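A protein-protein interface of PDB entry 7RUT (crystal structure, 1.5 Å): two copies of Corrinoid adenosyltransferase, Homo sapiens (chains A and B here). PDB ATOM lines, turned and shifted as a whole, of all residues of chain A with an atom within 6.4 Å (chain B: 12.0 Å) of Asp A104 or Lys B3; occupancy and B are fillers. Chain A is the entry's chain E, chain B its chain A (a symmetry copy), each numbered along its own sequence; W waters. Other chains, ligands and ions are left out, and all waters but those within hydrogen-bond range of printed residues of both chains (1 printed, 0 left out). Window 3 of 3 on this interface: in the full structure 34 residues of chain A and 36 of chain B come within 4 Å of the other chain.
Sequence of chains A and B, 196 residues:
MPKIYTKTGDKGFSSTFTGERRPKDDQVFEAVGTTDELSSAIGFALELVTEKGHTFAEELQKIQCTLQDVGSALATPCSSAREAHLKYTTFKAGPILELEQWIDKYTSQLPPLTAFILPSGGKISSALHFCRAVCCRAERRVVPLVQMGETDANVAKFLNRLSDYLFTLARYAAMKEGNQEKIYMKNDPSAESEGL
The side-chain carboxylate of Glu A100 lies within salt-bridge range of the side-chain amino group of Lys B7, at 3.8 Å.
The side-chain carboxylate of Asp A104 lies within salt-bridge range of the side-chain amino group of Lys B3, 3.4 Å away.
The side-chain carboxylate (OD1) of Asp A104 is in hydrogen-bond range of the side-chain hydroxyl (OH) of Tyr B5, 2.8 Å away.
O of Ile A103 is in hydrogen-bond range of OG1 of Thr A107, 2.8 Å away.
Among the printed residues, pairs that only touch across the chains: Glu A100 with Tyr B5 (3.6 Å), Ile A103 with Ile B4 (3.7 Å), Ile A103 with Tyr B5 (3.9 Å) and Thr A168 with Ile B4 (3.9 Å).
Printed residues of chain A within 4 Å of Lys B3: Asp A104.
Ile A103 touches just these residues of chain B: Ile B4 and Tyr B5.
No residue of chain B comes within 4 Å of Lys A105.
No residue of chain B comes within 4 Å of Ser A108.
Printed residues of chain B within 4 Å of Glu A100: Tyr B5 (3.6 Å) and Lys B7 (3.6 Å).
Of the printed residues of chain A, Lys B7 touches Glu A100 (3.6 Å).
Of the printed residues of chain A, Tyr B5 touches Glu A100, Ile A103 and Asp A104.
Printed residues of chain B that touch a printed residue of chain A: Lys B3, Ile B4, Tyr B5 and Lys B7.
Hydrophobic or aromatic side chains of chain B that line the printed part of chain A: Ile B4 and Tyr B5.
No position is printed for both chains.
Water W1 bridges OE2 of Glu A100 (2.9 Å) and NZ of Lys B7 (3.3 Å).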
ATOM      1  N   LEU A  99     -17.293   3.590  -9.703  1.00  0.00           N
ATOM      2  CA  LEU A  99     -17.081   4.058  -8.335  1.00  0.00           C
ATOM      3  C   LEU A  99     -15.805   4.884  -8.228  1.00  0.00           C
ATOM      4  O   LEU A  99     -15.775   5.907  -7.536  1.00  0.00           O
ATOM      5  CB  LEU A  99     -17.015   2.877  -7.363  1.00  0.00           C
ATOM      6  CG  LEU A  99     -18.311   2.194  -6.940  1.00  0.00           C
ATOM      7  CD1 LEU A  99     -17.975   1.122  -5.915  1.00  0.00           C
ATOM      8  CD2 LEU A  99     -19.328   3.187  -6.381  1.00  0.00           C
ATOM      9  N   GLU A 100     -14.736   4.442  -8.897  1.00  0.00           N
ATOM     10  CA  GLU A 100     -13.480   5.187  -8.868  1.00  0.00           C
ATOM     11  C   GLU A 100     -13.642   6.576  -9.471  1.00  0.00           C
ATOM     12  O   GLU A 100     -13.121   7.559  -8.932  1.00  0.00           O
ATOM     13  CB  GLU A 100     -12.389   4.398  -9.594  1.00  0.00           C
ATOM     14  CG  GLU A 100     -11.923   3.189  -8.776  1.00  0.00           C
ATOM     15  CD  GLU A 100     -11.141   2.169  -9.584  1.00  0.00           C
ATOM     16  OE1 GLU A 100     -10.687   2.505 -10.699  1.00  0.00           O
ATOM     17  OE2 GLU A 100     -10.982   1.027  -9.091  1.00  0.00           O
ATOM     18  N   GLN A 101     -14.360   6.679 -10.589  1.00  0.00           N
ATOM     19  CA  GLN A 101     -14.572   7.989 -11.195  1.00  0.00           C
ATOM     20  C   GLN A 101     -15.372   8.901 -10.276  1.00  0.00           C
ATOM     21  O   GLN A 101     -15.091  10.104 -10.187  1.00  0.00           O
ATOM     22  CB  GLN A 101     -15.264   7.830 -12.543  1.00  0.00           C
ATOM     23  CG  GLN A 101     -14.479   6.975 -13.517  1.00  0.00           C
ATOM     24  CD  GLN A 101     -15.131   6.901 -14.877  1.00  0.00           C
ATOM     25  OE1 GLN A 101     -14.842   7.707 -15.761  1.00  0.00           O
ATOM     26  NE2 GLN A 101     -16.026   5.935 -15.051  1.00  0.00           N
ATOM     27  N   TRP A 102     -16.368   8.345  -9.575  1.00  0.00           N
ATOM     28  CA  TRP A 102     -17.159   9.148  -8.647  1.00  0.00           C
ATOM     29  C   TRP A 102     -16.320   9.580  -7.452  1.00  0.00           C
ATOM     30  O   TRP A 102     -16.381  10.737  -7.030  1.00  0.00           O
ATOM     31  CB  TRP A 102     -18.393   8.374  -8.181  1.00  0.00           C
ATOM     32  CG  TRP A 102     -19.409   8.131  -9.246  1.00  0.00           C
ATOM     33  CD1 TRP A 102     -19.471   8.713 -10.482  1.00  0.00           C
ATOM     34  CD2 TRP A 102     -20.511   7.223  -9.175  1.00  0.00           C
ATOM     35  NE1 TRP A 102     -20.548   8.225 -11.181  1.00  0.00           N
ATOM     36  CE2 TRP A 102     -21.201   7.305 -10.400  1.00  0.00           C
ATOM     37  CE3 TRP A 102     -20.980   6.348  -8.193  1.00  0.00           C
ATOM     38  CZ2 TRP A 102     -22.345   6.549 -10.664  1.00  0.00           C
ATOM     39  CZ3 TRP A 102     -22.115   5.599  -8.456  1.00  0.00           C
ATOM     40  CH2 TRP A 102     -22.779   5.696  -9.680  1.00  0.00           C
ATOM     41  N   ILE A 103     -15.542   8.654  -6.878  1.00  0.00           N
ATOM     42  CA  ILE A 103     -14.640   9.024  -5.789  1.00  0.00           C
ATOM     43  C   ILE A 103     -13.725  10.170  -6.217  1.00  0.00           C
ATOM     44  O   ILE A 103     -13.523  11.140  -5.477  1.00  0.00           O
ATOM     45  CB  ILE A 103     -13.819   7.806  -5.332  1.00  0.00           C
ATOM     46  CG1 ILE A 103     -14.701   6.775  -4.618  1.00  0.00           C
ATOM     47  CG2 ILE A 103     -12.673   8.249  -4.437  1.00  0.00           C
ATOM     48  CD1 ILE A 103     -14.017   5.435  -4.419  1.00  0.00           C
ATOM     49  N   ASP A 104     -13.151  10.067  -7.420  1.00  0.00           N
ATOM     50  CA  ASP A 104     -12.273  11.121  -7.932  1.00  0.00           C
ATOM     51  C   ASP A 104     -13.003  12.453  -8.034  1.00  0.00           C
ATOM     52  O   ASP A 104     -12.434  13.508  -7.720  1.00  0.00           O
ATOM     53  CB  ASP A 104     -11.724  10.728  -9.301  1.00  0.00           C
ATOM     54  CG  ASP A 104     -10.746   9.567  -9.239  1.00  0.00           C
ATOM     55  OD1 ASP A 104     -10.398   9.111  -8.126  1.00  0.00           O
ATOM     56  OD2 ASP A 104     -10.324   9.114 -10.322  1.00  0.00           O
ATOM     57  N   LYS A 105     -14.253  12.424  -8.500  1.00  0.00           N
ATOM     58  CA  LYS A 105     -15.036  13.646  -8.653  1.00  0.00           C
ATOM     59  C   LYS A 105     -15.217  14.355  -7.314  1.00  0.00           C
ATOM     60  O   LYS A 105     -14.990  15.566  -7.201  1.00  0.00           O
ATOM     61  CB  LYS A 105     -16.390  13.314  -9.281  1.00  0.00           C
ATOM     62  CG  LYS A 105     -17.406  14.445  -9.213  1.00  0.00           C
ATOM     63  CD  LYS A 105     -18.748  14.038  -9.830  1.00  0.00           C
ATOM     64  CE  LYS A 105     -19.372  12.866  -9.091  1.00  0.00           C
ATOM     65  NZ  LYS A 105     -20.740  12.538  -9.592  1.00  0.00           N
ATOM     66  N   TYR A 106     -15.617  13.611  -6.279  1.00  0.00           N
ATOM     67  CA  TYR A 106     -15.849  14.238  -4.983  1.00  0.00           C
ATOM     68  C   TYR A 106     -14.538  14.626  -4.321  1.00  0.00           C
ATOM     69  O   TYR A 106     -14.460  15.659  -3.648  1.00  0.00           O
ATOM     70  CB  TYR A 106     -16.657  13.295  -4.086  1.00  0.00           C
ATOM     71  CG  TYR A 106     -18.028  13.022  -4.657  1.00  0.00           C
ATOM     72  CD1 TYR A 106     -18.872  14.070  -5.004  1.00  0.00           C
ATOM     73  CD2 TYR A 106     -18.474  11.721  -4.870  1.00  0.00           C
ATOM     74  CE1 TYR A 106     -20.129  13.836  -5.540  1.00  0.00           C
ATOM     75  CE2 TYR A 106     -19.729  11.474  -5.409  1.00  0.00           C
ATOM     76  CZ  TYR A 106     -20.552  12.540  -5.743  1.00  0.00           C
ATOM     77  OH  TYR A 106     -21.795  12.310  -6.278  1.00  0.00           O
ATOM     78  N   THR A 107     -13.501  13.805  -4.500  1.00  0.00           N
ATOM     79  CA  THR A 107     -12.198  14.117  -3.930  1.00  0.00           C
ATOM     80  C   THR A 107     -11.663  15.436  -4.478  1.00  0.00           C
ATOM     81  O   THR A 107     -11.037  16.211  -3.745  1.00  0.00           O
ATOM     82  CB  THR A 107     -11.228  12.963  -4.203  1.00  0.00           C
ATOM     83  OG1 THR A 107     -11.687  11.788  -3.508  1.00  0.00           O
ATOM     84  CG2 THR A 107      -9.836  13.300  -3.723  1.00  0.00           C
ATOM     85  N   SER A 108     -11.932  15.728  -5.752  1.00  0.00           N
ATOM     86  CA  SER A 108     -11.489  16.988  -6.343  1.00  0.00           C
ATOM     87  C   SER A 108     -12.199  18.202  -5.757  1.00  0.00           C
ATOM     88  O   SER A 108     -11.743  19.329  -5.983  1.00  0.00           O
ATOM     89  CB  SER A 108     -11.697  16.965  -7.860  1.00  0.00           C
ATOM     90  OG  SER A 108     -13.078  17.001  -8.190  1.00  0.00           O
ATOM     91  N   GLN A 109     -13.291  18.010  -5.017  1.00  0.00           N
ATOM     92  CA  GLN A 109     -14.025  19.109  -4.404  1.00  0.00           C
ATOM     93  C   GLN A 109     -13.788  19.217  -2.904  1.00  0.00           C
ATOM     94  O   GLN A 109     -14.486  19.982  -2.233  1.00  0.00           O
ATOM     95  CB  GLN A 109     -15.525  18.959  -4.665  1.00  0.00           C
ATOM     96  CG  GLN A 109     -15.914  18.863  -6.124  1.00  0.00           C
ATOM     97  CD  GLN A 109     -17.419  18.786  -6.312  1.00  0.00           C
ATOM     98  OE1 GLN A 109     -18.136  19.760  -6.083  1.00  0.00           O
ATOM     99  NE2 GLN A 109     -17.907  17.617  -6.722  1.00  0.00           N
ATOM    100  N   THR A 168     -16.102   8.795   1.217  1.00  0.00           N
ATOM    101  CA  THR A 168     -15.880  10.061   0.517  1.00  0.00           C
ATOM    102  C   THR A 168     -17.182  10.841   0.371  1.00  0.00           C
ATOM    103  O   THR A 168     -17.201  12.074   0.515  1.00  0.00           O
ATOM    104  CB  THR A 168     -15.256   9.802  -0.857  1.00  0.00           C
ATOM    105  OG1 THR A 168     -14.054   9.039  -0.710  1.00  0.00           O
ATOM    106  CG2 THR A 168     -14.937  11.132  -1.569  1.00  0.00           C
ATOM    107  N   PRO B   2      -1.998  10.558  -3.229  1.00  0.00           N
ATOM    108  CA  PRO B   2      -2.391   9.155  -3.372  1.00  0.00           C
ATOM    109  C   PRO B   2      -3.887   8.955  -3.178  1.00  0.00           C
ATOM    110  O   PRO B   2      -4.468   9.495  -2.237  1.00  0.00           O
ATOM    111  CB  PRO B   2      -1.609   8.453  -2.255  1.00  0.00           C
ATOM    112  CG  PRO B   2      -1.129   9.569  -1.321  1.00  0.00           C
ATOM    113  CD  PRO B   2      -1.656  10.876  -1.835  1.00  0.00           C
ATOM    114  N   LYS B   3      -4.498   8.172  -4.059  1.00  0.00           N
ATOM    115  CA  LYS B   3      -5.934   7.970  -3.993  1.00  0.00           C
ATOM    116  C   LYS B   3      -6.303   7.109  -2.793  1.00  0.00           C
ATOM    117  O   LYS B   3      -5.514   6.285  -2.323  1.00  0.00           O
ATOM    118  CB  LYS B   3      -6.429   7.335  -5.289  1.00  0.00           C
ATOM    119  CG  LYS B   3      -6.064   8.160  -6.516  1.00  0.00           C
ATOM    120  CD  LYS B   3      -6.925   7.809  -7.703  1.00  0.00           C
ATOM    121  CE  LYS B   3      -6.727   8.770  -8.869  1.00  0.00           C
ATOM    122  NZ  LYS B   3      -7.224  10.148  -8.581  1.00  0.00           N
ATOM    123  N   ILE B   4      -7.524   7.324  -2.291  1.00  0.00           N
ATOM    124  CA  ILE B   4      -8.015   6.584  -1.131  1.00  0.00           C
ATOM    125  C   ILE B   4      -8.048   5.089  -1.411  1.00  0.00           C
ATOM    126  O   ILE B   4      -7.844   4.269  -0.500  1.00  0.00           O
ATOM    127  CB  ILE B   4      -9.403   7.118  -0.722  1.00  0.00           C
ATOM    128  CG1 ILE B   4      -9.876   6.473   0.581  1.00  0.00           C
ATOM    129  CG2 ILE B   4     -10.437   6.879  -1.828  1.00  0.00           C
ATOM    130  CD1 ILE B   4     -11.257   6.937   1.002  1.00  0.00           C
ATOM    131  N   TYR B   5      -8.296   4.703  -2.660  1.00  0.00           N
ATOM    132  CA  TYR B   5      -8.330   3.288  -3.019  1.00  0.00           C
ATOM    133  C   TYR B   5      -6.927   2.888  -3.460  1.00  0.00           C
ATOM    134  O   TYR B   5      -6.508   3.179  -4.585  1.00  0.00           O
ATOM    135  CB  TYR B   5      -9.381   3.007  -4.091  1.00  0.00           C
ATOM    136  CG  TYR B   5      -9.414   3.952  -5.275  1.00  0.00           C
ATOM    137  CD1 TYR B   5     -10.080   5.172  -5.203  1.00  0.00           C
ATOM    138  CD2 TYR B   5      -8.808   3.609  -6.479  1.00  0.00           C
ATOM    139  CE1 TYR B   5     -10.109   6.038  -6.293  1.00  0.00           C
ATOM    140  CE2 TYR B   5      -8.834   4.466  -7.571  1.00  0.00           C
ATOM    141  CZ  TYR B   5      -9.496   5.675  -7.474  1.00  0.00           C
ATOM    142  OH  TYR B   5      -9.528   6.523  -8.560  1.00  0.00           O
ATOM    143  N   THR B   6      -6.176   2.254  -2.550  1.00  0.00           N
ATOM    144  CA  THR B   6      -4.851   1.753  -2.895  1.00  0.00           C
ATOM    145  C   THR B   6      -4.927   0.477  -3.713  1.00  0.00           C
ATOM    146  O   THR B   6      -3.969   0.148  -4.418  1.00  0.00           O
ATOM    147  CB  THR B   6      -4.017   1.474  -1.639  1.00  0.00           C
ATOM    148  OG1 THR B   6      -4.528   0.308  -0.971  1.00  0.00           O
ATOM    149  CG2 THR B   6      -4.039   2.658  -0.685  1.00  0.00           C
ATOM    150  N   LYS B   7      -6.045  -0.245  -3.621  1.00  0.00           N
ATOM    151  CA  LYS B   7      -6.290  -1.546  -4.235  1.00  0.00           C
ATOM    152  C   LYS B   7      -5.474  -2.659  -3.587  1.00  0.00           C
ATOM    153  O   LYS B   7      -5.577  -3.813  -4.019  1.00  0.00           O
ATOM    154  CB  LYS B   7      -6.032  -1.526  -5.747  1.00  0.00           C
ATOM    155  CG  LYS B   7      -6.863  -0.464  -6.471  1.00  0.00           C
ATOM    156  CD  LYS B   7      -6.785  -0.645  -7.964  1.00  0.00           C
ATOM    157  CE  LYS B   7      -7.397   0.538  -8.698  1.00  0.00           C
ATOM    158  NZ  LYS B   7      -7.434   0.268 -10.159  1.00  0.00           N
ATOM    159  N   THR B   8      -4.684  -2.368  -2.550  1.00  0.00           N
ATOM    160  CA  THR B   8      -3.925  -3.430  -1.892  1.00  0.00           C
ATOM    161  C   THR B   8      -4.824  -4.384  -1.114  1.00  0.00           C
ATOM    162  O   THR B   8      -4.386  -5.493  -0.777  1.00  0.00           O
ATOM    163  CB  THR B   8      -2.866  -2.843  -0.955  1.00  0.00           C
ATOM    164  OG1 THR B   8      -3.491  -2.014   0.031  1.00  0.00           O
ATOM    165  CG2 THR B   8      -1.855  -2.012  -1.738  1.00  0.00           C
ATOM    166  N   GLY B   9      -6.057  -3.977  -0.809  1.00  0.00           N
ATOM    167  CA  GLY B   9      -7.039  -4.818  -0.158  1.00  0.00           C
ATOM    168  C   GLY B   9      -7.945  -5.555  -1.114  1.00  0.00           C
ATOM    169  O   GLY B   9      -8.884  -6.233  -0.684  1.00  0.00           O
ATOM    170  N   ASP B  10      -7.672  -5.463  -2.411  1.00  0.00           N
ATOM    171  CA  ASP B  10      -8.577  -5.955  -3.439  1.00  0.00           C
ATOM    172  C   ASP B  10      -8.607  -7.481  -3.518  1.00  0.00           C
ATOM    173  O   ASP B  10      -9.583  -8.045  -4.021  1.00  0.00           O
ATOM    174  CB  ASP B  10      -8.161  -5.362  -4.784  1.00  0.00           C
ATOM    175  CG  ASP B  10      -8.974  -4.136  -5.157  1.00  0.00           C
ATOM    176  OD1 ASP B  10      -8.898  -3.708  -6.336  1.00  0.00           O
ATOM    177  OD2 ASP B  10      -9.686  -3.607  -4.279  1.00  0.00           O
HETATM  178  O   HOH W   1     -10.225  -1.434 -10.482  1.00  0.00           O
